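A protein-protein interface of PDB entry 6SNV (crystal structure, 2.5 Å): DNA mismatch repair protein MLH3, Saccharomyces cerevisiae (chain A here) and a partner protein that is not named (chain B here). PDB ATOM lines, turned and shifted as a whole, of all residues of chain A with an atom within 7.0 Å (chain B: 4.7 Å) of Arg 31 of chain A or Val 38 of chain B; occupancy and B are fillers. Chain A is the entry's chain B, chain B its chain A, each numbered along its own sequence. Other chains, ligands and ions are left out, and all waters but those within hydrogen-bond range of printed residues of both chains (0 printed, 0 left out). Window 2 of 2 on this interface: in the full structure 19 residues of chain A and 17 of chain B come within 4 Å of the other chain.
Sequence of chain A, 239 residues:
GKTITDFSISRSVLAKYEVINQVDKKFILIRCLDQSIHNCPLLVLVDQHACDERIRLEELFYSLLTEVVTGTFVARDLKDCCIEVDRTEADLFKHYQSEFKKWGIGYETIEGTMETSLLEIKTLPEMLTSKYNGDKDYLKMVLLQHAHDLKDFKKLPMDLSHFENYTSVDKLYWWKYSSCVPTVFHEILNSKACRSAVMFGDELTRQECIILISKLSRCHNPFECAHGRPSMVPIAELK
The guanidinium group (NH2) of Arg 31 of chain A is in salt-bridge range of the side-chain carboxylate (OE1) of Glu 40 of chain B (3.0 Å). O of Val 38 of chain B sits at hydrogen-bond distance from NH1 of Arg 31 of chain A, 2.9 Å away.
The backbone NH (N) of Ile 20 of chain A sits at hydrogen-bond distance from the backbone carbonyl oxygen (O) of Leu 29 of chain A (2.8 Å). The backbone carbonyl oxygen of Leu 44 of chain B sits at hydrogen-bond distance from the backbone NH of Val 38 of chain B, at 2.9 Å. The backbone carbonyl oxygen (O) of Gly 36 of chain B is in hydrogen-bond range of the backbone NH (N) of Ala 46 of chain B (2.8 Å). The side-chain carboxylate of Glu 18 of chain A lies within salt-bridge range of the guanidinium group of Arg 31 of chain A (3.4 Å).
CA of Gly 36 of chain B touches CG2 of Ile 20 of chain A, at 3.7 Å. Ile 20 of chain A touches Val 37 of chain B (CG1 to O, 3.3 Å). Ile 20 of chain A touches Val 38 of chain B. Arg 31 of chain A touches Val 37 of chain B. CG1 of Val 38 of chain B touches CD2 of Leu 43 of chain A (3.9 Å).
Glu 18 of chain A touches none of the printed residues of chain B. Of the printed residues of chain B, Ile 20 of chain A touches Gly 36 (3.7 Å), Val 37 (3.3 Å) and Val 38 (3.8 Å). Arg 31 of chain A touches just these residues of chain B: Val 37, Val 38 and Glu 40. Of the printed residues of chain B, Leu 43 of chain A touches Val 38 (3.9 Å). Val 44 of chain A touches none of the printed residues of chain B. Of the printed residues of chain A, Gly 36 of chain B touches Ile 20. Of the printed residues of chain A, Val 37 of chain B touches Ile 20 (3.3 Å) and Arg 31 (3.6 Å). Val 38 of chain B touches just these residues of chain A: Ile 20, Arg 31 and Leu 43. Printed residues of chain A within 4 Å of Glu 40 of chain B: Arg 31.
Of the 9 printed residues of chain B, 4 touch a printed residue of chain A. Hydrophobic or aromatic side chains of chain B that line the printed part of chain A: Val 38. Printed residues of chain A that touch a printed residue of chain B: Ile 20, Arg 31 and Leu 43. Hydrophobic or aromatic side chains of chain A within 4 Å of the printed part of chain B: Ile 20 and Leu 43. Among the printed residues, 7 pairs touch across the chains. Among the printed residues, Asp or Glu carboxylates within 4 Å of a Lys or Arg side-chain nitrogen of the other chain: Arg 31 of chain A with Glu 40 of chain B (3.0 Å).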
ATOM      1  N   LYS A  16     -35.859 -29.148 -19.146  1.00  0.00           N
ATOM      2  CA  LYS A  16     -34.651 -29.857 -19.581  1.00  0.00           C
ATOM      3  C   LYS A  16     -33.421 -28.911 -19.633  1.00  0.00           C
ATOM      4  O   LYS A  16     -32.630 -28.954 -20.579  1.00  0.00           O
ATOM      5  CB  LYS A  16     -34.895 -30.573 -20.928  1.00  0.00           C
ATOM      6  CG  LYS A  16     -35.721 -31.861 -20.832  1.00  0.00           C
ATOM      7  CD  LYS A  16     -34.839 -33.112 -20.776  1.00  0.00           C
ATOM      8  CE  LYS A  16     -35.621 -34.398 -20.927  1.00  0.00           C
ATOM      9  NZ  LYS A  16     -35.939 -34.697 -22.348  1.00  0.00           N
ATOM     10  N   TYR A  17     -33.265 -28.064 -18.592  1.00  0.00           N
ATOM     11  CA  TYR A  17     -32.177 -27.089 -18.472  1.00  0.00           C
ATOM     12  C   TYR A  17     -31.340 -27.270 -17.208  1.00  0.00           C
ATOM     13  O   TYR A  17     -31.896 -27.456 -16.124  1.00  0.00           O
ATOM     14  CB  TYR A  17     -32.705 -25.641 -18.565  1.00  0.00           C
ATOM     15  CG  TYR A  17     -32.662 -25.059 -19.964  1.00  0.00           C
ATOM     16  CD1 TYR A  17     -33.659 -25.341 -20.892  1.00  0.00           C
ATOM     17  CD2 TYR A  17     -31.638 -24.201 -20.351  1.00  0.00           C
ATOM     18  CE1 TYR A  17     -33.628 -24.802 -22.177  1.00  0.00           C
ATOM     19  CE2 TYR A  17     -31.600 -23.648 -21.631  1.00  0.00           C
ATOM     20  CZ  TYR A  17     -32.597 -23.953 -22.542  1.00  0.00           C
ATOM     21  OH  TYR A  17     -32.557 -23.432 -23.811  1.00  0.00           O
ATOM     22  N   GLU A  18     -30.002 -27.204 -17.360  1.00  0.00           N
ATOM     23  CA  GLU A  18     -29.020 -27.308 -16.281  1.00  0.00           C
ATOM     24  C   GLU A  18     -28.364 -25.942 -16.049  1.00  0.00           C
ATOM     25  O   GLU A  18     -28.086 -25.220 -17.010  1.00  0.00           O
ATOM     26  CB  GLU A  18     -27.958 -28.373 -16.600  1.00  0.00           C
ATOM     27  CG  GLU A  18     -27.552 -29.188 -15.382  1.00  0.00           C
ATOM     28  CD  GLU A  18     -26.077 -29.519 -15.245  1.00  0.00           C
ATOM     29  OE1 GLU A  18     -25.767 -30.657 -14.821  1.00  0.00           O
ATOM     30  OE2 GLU A  18     -25.231 -28.644 -15.541  1.00  0.00           O
ATOM     31  N   VAL A  19     -28.146 -25.582 -14.774  1.00  0.00           N
ATOM     32  CA  VAL A  19     -27.557 -24.292 -14.396  1.00  0.00           C
ATOM     33  C   VAL A  19     -26.048 -24.336 -14.573  1.00  0.00           C
ATOM     34  O   VAL A  19     -25.409 -25.276 -14.103  1.00  0.00           O
ATOM     35  CB  VAL A  19     -27.967 -23.885 -12.943  1.00  0.00           C
ATOM     36  CG1 VAL A  19     -27.108 -22.749 -12.382  1.00  0.00           C
ATOM     37  CG2 VAL A  19     -29.440 -23.521 -12.872  1.00  0.00           C
ATOM     38  N   ILE A  20     -25.475 -23.314 -15.225  1.00  0.00           N
ATOM     39  CA  ILE A  20     -24.026 -23.199 -15.327  1.00  0.00           C
ATOM     40  C   ILE A  20     -23.571 -22.481 -14.032  1.00  0.00           C
ATOM     41  O   ILE A  20     -23.124 -23.159 -13.108  1.00  0.00           O
ATOM     42  CB  ILE A  20     -23.543 -22.600 -16.682  1.00  0.00           C
ATOM     43  CG1 ILE A  20     -23.784 -23.636 -17.801  1.00  0.00           C
ATOM     44  CG2 ILE A  20     -22.064 -22.183 -16.630  1.00  0.00           C
ATOM     45  CD1 ILE A  20     -23.633 -23.172 -19.152  1.00  0.00           C
ATOM     46  N   LEU A  29     -26.643 -18.075 -16.009  1.00  0.00           N
ATOM     47  CA  LEU A  29     -26.409 -18.731 -17.289  1.00  0.00           C
ATOM     48  C   LEU A  29     -26.837 -20.183 -17.155  1.00  0.00           C
ATOM     49  O   LEU A  29     -26.409 -20.868 -16.222  1.00  0.00           O
ATOM     50  CB  LEU A  29     -24.937 -18.597 -17.730  1.00  0.00           C
ATOM     51  CG  LEU A  29     -24.540 -19.252 -19.062  1.00  0.00           C
ATOM     52  CD1 LEU A  29     -25.108 -18.498 -20.252  1.00  0.00           C
ATOM     53  CD2 LEU A  29     -23.037 -19.368 -19.180  1.00  0.00           C
ATOM     54  N   ILE A  30     -27.733 -20.622 -18.056  1.00  0.00           N
ATOM     55  CA  ILE A  30     -28.292 -21.978 -18.114  1.00  0.00           C
ATOM     56  C   ILE A  30     -28.019 -22.650 -19.483  1.00  0.00           C
ATOM     57  O   ILE A  30     -27.830 -21.960 -20.489  1.00  0.00           O
ATOM     58  CB  ILE A  30     -29.803 -22.012 -17.709  1.00  0.00           C
ATOM     59  CG1 ILE A  30     -30.676 -21.100 -18.608  1.00  0.00           C
ATOM     60  CG2 ILE A  30     -29.988 -21.687 -16.225  1.00  0.00           C
ATOM     61  CD1 ILE A  30     -32.220 -21.328 -18.577  1.00  0.00           C
ATOM     62  N   ARG A  31     -27.987 -23.992 -19.508  1.00  0.00           N
ATOM     63  CA  ARG A  31     -27.760 -24.789 -20.720  1.00  0.00           C
ATOM     64  C   ARG A  31     -28.842 -25.851 -20.892  1.00  0.00           C
ATOM     65  O   ARG A  31     -29.244 -26.456 -19.905  1.00  0.00           O
ATOM     66  CB  ARG A  31     -26.354 -25.433 -20.737  1.00  0.00           C
ATOM     67  CG  ARG A  31     -25.988 -26.225 -19.484  1.00  0.00           C
ATOM     68  CD  ARG A  31     -25.096 -27.401 -19.792  1.00  0.00           C
ATOM     69  NE  ARG A  31     -24.233 -27.724 -18.655  1.00  0.00           N
ATOM     70  CZ  ARG A  31     -23.298 -28.670 -18.663  1.00  0.00           C
ATOM     71  NH1 ARG A  31     -23.098 -29.406 -19.749  1.00  0.00           N
ATOM     72  NH2 ARG A  31     -22.559 -28.887 -17.585  1.00  0.00           N
ATOM     73  N   CYS A  32     -29.312 -26.075 -22.135  1.00  0.00           N
ATOM     74  CA  CYS A  32     -30.352 -27.061 -22.463  1.00  0.00           C
ATOM     75  C   CYS A  32     -29.877 -28.512 -22.278  1.00  0.00           C
ATOM     76  O   CYS A  32     -28.774 -28.871 -22.690  1.00  0.00           O
ATOM     77  CB  CYS A  32     -30.898 -26.820 -23.868  1.00  0.00           C
ATOM     78  SG  CYS A  32     -32.291 -27.885 -24.321  1.00  0.00           S
ATOM     79  N   LEU A  42     -29.717 -23.304 -26.879  1.00  0.00           N
ATOM     80  CA  LEU A  42     -28.737 -23.999 -26.040  1.00  0.00           C
ATOM     81  C   LEU A  42     -28.355 -23.209 -24.780  1.00  0.00           C
ATOM     82  O   LEU A  42     -28.534 -23.737 -23.686  1.00  0.00           O
ATOM     83  CB  LEU A  42     -27.477 -24.433 -26.825  1.00  0.00           C
ATOM     84  CG  LEU A  42     -26.448 -25.275 -26.026  1.00  0.00           C
ATOM     85  CD1 LEU A  42     -26.582 -26.760 -26.340  1.00  0.00           C
ATOM     86  CD2 LEU A  42     -25.010 -24.799 -26.265  1.00  0.00           C
ATOM     87  N   LEU A  43     -27.792 -21.987 -24.921  1.00  0.00           N
ATOM     88  CA  LEU A  43     -27.422 -21.167 -23.759  1.00  0.00           C
ATOM     89  C   LEU A  43     -28.403 -20.024 -23.582  1.00  0.00           C
ATOM     90  O   LEU A  43     -28.679 -19.289 -24.530  1.00  0.00           O
ATOM     91  CB  LEU A  43     -25.978 -20.626 -23.816  1.00  0.00           C
ATOM     92  CG  LEU A  43     -24.815 -21.623 -23.746  1.00  0.00           C
ATOM     93  CD1 LEU A  43     -23.495 -20.905 -23.864  1.00  0.00           C
ATOM     94  CD2 LEU A  43     -24.828 -22.421 -22.459  1.00  0.00           C
ATOM     95  N   VAL A  44     -28.953 -19.893 -22.374  1.00  0.00           N
ATOM     96  CA  VAL A  44     -29.921 -18.855 -22.047  1.00  0.00           C
ATOM     97  C   VAL A  44     -29.431 -18.078 -20.816  1.00  0.00           C
ATOM     98  O   VAL A  44     -28.920 -18.678 -19.867  1.00  0.00           O
ATOM     99  CB  VAL A  44     -31.355 -19.442 -21.859  1.00  0.00           C
ATOM    100  CG1 VAL A  44     -32.373 -18.351 -21.545  1.00  0.00           C
ATOM    101  CG2 VAL A  44     -31.803 -20.237 -23.082  1.00  0.00           C
ATOM    102  N   ARG A 206     -24.129 -21.200  -6.616  1.00  0.00           N
ATOM    103  CA  ARG A 206     -24.689 -22.091  -7.647  1.00  0.00           C
ATOM    104  C   ARG A 206     -25.941 -22.790  -7.103  1.00  0.00           C
ATOM    105  O   ARG A 206     -26.925 -22.893  -7.830  1.00  0.00           O
ATOM    106  CB  ARG A 206     -23.670 -23.114  -8.177  1.00  0.00           C
ATOM    107  CG  ARG A 206     -23.958 -23.515  -9.623  1.00  0.00           C
ATOM    108  CD  ARG A 206     -23.005 -24.548 -10.199  1.00  0.00           C
ATOM    109  NE  ARG A 206     -23.359 -25.913  -9.799  1.00  0.00           N
ATOM    110  CZ  ARG A 206     -24.035 -26.780 -10.551  1.00  0.00           C
ATOM    111  NH1 ARG A 206     -24.468 -26.429 -11.758  1.00  0.00           N
ATOM    112  NH2 ARG A 206     -24.297 -28.004 -10.099  1.00  0.00           N
ATOM    113  N   GLY B  36     -18.276 -21.278 -15.726  1.00  0.00           N
ATOM    114  CA  GLY B  36     -18.532 -22.706 -15.547  1.00  0.00           C
ATOM    115  C   GLY B  36     -18.487 -23.557 -16.804  1.00  0.00           C
ATOM    116  O   GLY B  36     -18.228 -23.049 -17.897  1.00  0.00           O
ATOM    117  N   VAL B  37     -18.750 -24.870 -16.651  1.00  0.00           N
ATOM    118  CA  VAL B  37     -18.743 -25.814 -17.771  1.00  0.00           C
ATOM    119  C   VAL B  37     -20.006 -25.677 -18.612  1.00  0.00           C
ATOM    120  O   VAL B  37     -21.110 -25.623 -18.072  1.00  0.00           O
ATOM    121  CB  VAL B  37     -18.481 -27.290 -17.351  1.00  0.00           C
ATOM    122  CG1 VAL B  37     -18.302 -28.196 -18.575  1.00  0.00           C
ATOM    123  CG2 VAL B  37     -17.259 -27.401 -16.445  1.00  0.00           C
ATOM    124  N   VAL B  38     -19.829 -25.653 -19.936  1.00  0.00           N
ATOM    125  CA  VAL B  38     -20.890 -25.567 -20.938  1.00  0.00           C
ATOM    126  C   VAL B  38     -21.142 -26.961 -21.537  1.00  0.00           C
ATOM    127  O   VAL B  38     -22.293 -27.370 -21.623  1.00  0.00           O
ATOM    128  CB  VAL B  38     -20.570 -24.478 -22.004  1.00  0.00           C
ATOM    129  CG1 VAL B  38     -21.581 -24.487 -23.151  1.00  0.00           C
ATOM    130  CG2 VAL B  38     -20.489 -23.094 -21.360  1.00  0.00           C
ATOM    131  N   ASP B  39     -20.075 -27.693 -21.928  1.00  0.00           N
ATOM    132  CA  ASP B  39     -20.182 -29.039 -22.507  1.00  0.00           C
ATOM    133  C   ASP B  39     -18.990 -29.922 -22.119  1.00  0.00           C
ATOM    134  O   ASP B  39     -17.879 -29.686 -22.593  1.00  0.00           O
ATOM    135  CB  ASP B  39     -20.331 -28.956 -24.042  1.00  0.00           C
ATOM    136  CG  ASP B  39     -20.860 -30.201 -24.741  1.00  0.00           C
ATOM    137  OD1 ASP B  39     -20.784 -31.303 -24.146  1.00  0.00           O
ATOM    138  OD2 ASP B  39     -21.337 -30.077 -25.895  1.00  0.00           O
ATOM    139  N   GLU B  40     -19.227 -30.951 -21.280  1.00  0.00           N
ATOM    140  CA  GLU B  40     -18.188 -31.897 -20.829  1.00  0.00           C
ATOM    141  C   GLU B  40     -17.661 -32.828 -21.939  1.00  0.00           C
ATOM    142  O   GLU B  40     -16.553 -33.353 -21.810  1.00  0.00           O
ATOM    143  CB  GLU B  40     -18.660 -32.725 -19.620  1.00  0.00           C
ATOM    144  CG  GLU B  40     -18.857 -31.928 -18.339  1.00  0.00           C
ATOM    145  CD  GLU B  40     -20.271 -31.465 -18.024  1.00  0.00           C
ATOM    146  OE1 GLU B  40     -20.476 -30.921 -16.913  1.00  0.00           O
ATOM    147  OE2 GLU B  40     -21.173 -31.648 -18.876  1.00  0.00           O
ATOM    148  N   LEU B  44     -16.201 -27.643 -23.510  1.00  0.00           N
ATOM    149  CA  LEU B  44     -16.480 -26.206 -23.550  1.00  0.00           C
ATOM    150  C   LEU B  44     -16.740 -25.644 -22.165  1.00  0.00           C
ATOM    151  O   LEU B  44     -17.387 -26.288 -21.337  1.00  0.00           O
ATOM    152  CB  LEU B  44     -17.663 -25.874 -24.469  1.00  0.00           C
ATOM    153  CG  LEU B  44     -17.597 -26.322 -25.932  1.00  0.00           C
ATOM    154  CD1 LEU B  44     -18.930 -26.115 -26.597  1.00  0.00           C
ATOM    155  CD2 LEU B  44     -16.508 -25.585 -26.708  1.00  0.00           C
ATOM    156  N   ALA B  45     -16.222 -24.438 -21.921  1.00  0.00           N
ATOM    157  CA  ALA B  45     -16.350 -23.700 -20.672  1.00  0.00           C
ATOM    158  C   ALA B  45     -16.668 -22.242 -20.998  1.00  0.00           C
ATOM    159  O   ALA B  45     -16.383 -21.786 -22.108  1.00  0.00           O
ATOM    160  CB  ALA B  45     -15.053 -23.788 -19.889  1.00  0.00           C
ATOM    161  N   ALA B  46     -17.283 -21.515 -20.052  1.00  0.00           N
ATOM    162  CA  ALA B  46     -17.620 -20.110 -20.258  1.00  0.00           C
ATOM    163  C   ALA B  46     -16.826 -19.233 -19.319  1.00  0.00           C
ATOM    164  O   ALA B  46     -16.612 -19.594 -18.159  1.00  0.00           O
ATOM    165  CB  ALA B  46     -19.107 -19.877 -20.076  1.00  0.00           C
ATOM    166  N   LEU B  55     -17.043 -18.265 -25.012  1.00  0.00           N
ATOM    167  CA  LEU B  55     -17.102 -19.718 -25.056  1.00  0.00           C
ATOM    168  C   LEU B  55     -15.693 -20.208 -25.408  1.00  0.00           C
ATOM    169  O   LEU B  55     -15.148 -19.826 -26.447  1.00  0.00           O
ATOM    170  CB  LEU B  55     -18.132 -20.186 -26.084  1.00  0.00           C
ATOM    171  CG  LEU B  55     -18.527 -21.654 -26.003  1.00  0.00           C
ATOM    172  CD1 LEU B  55     -19.320 -21.947 -24.742  1.00  0.00           C
ATOM    173  CD2 LEU B  55     -19.328 -22.054 -27.210  1.00  0.00           C
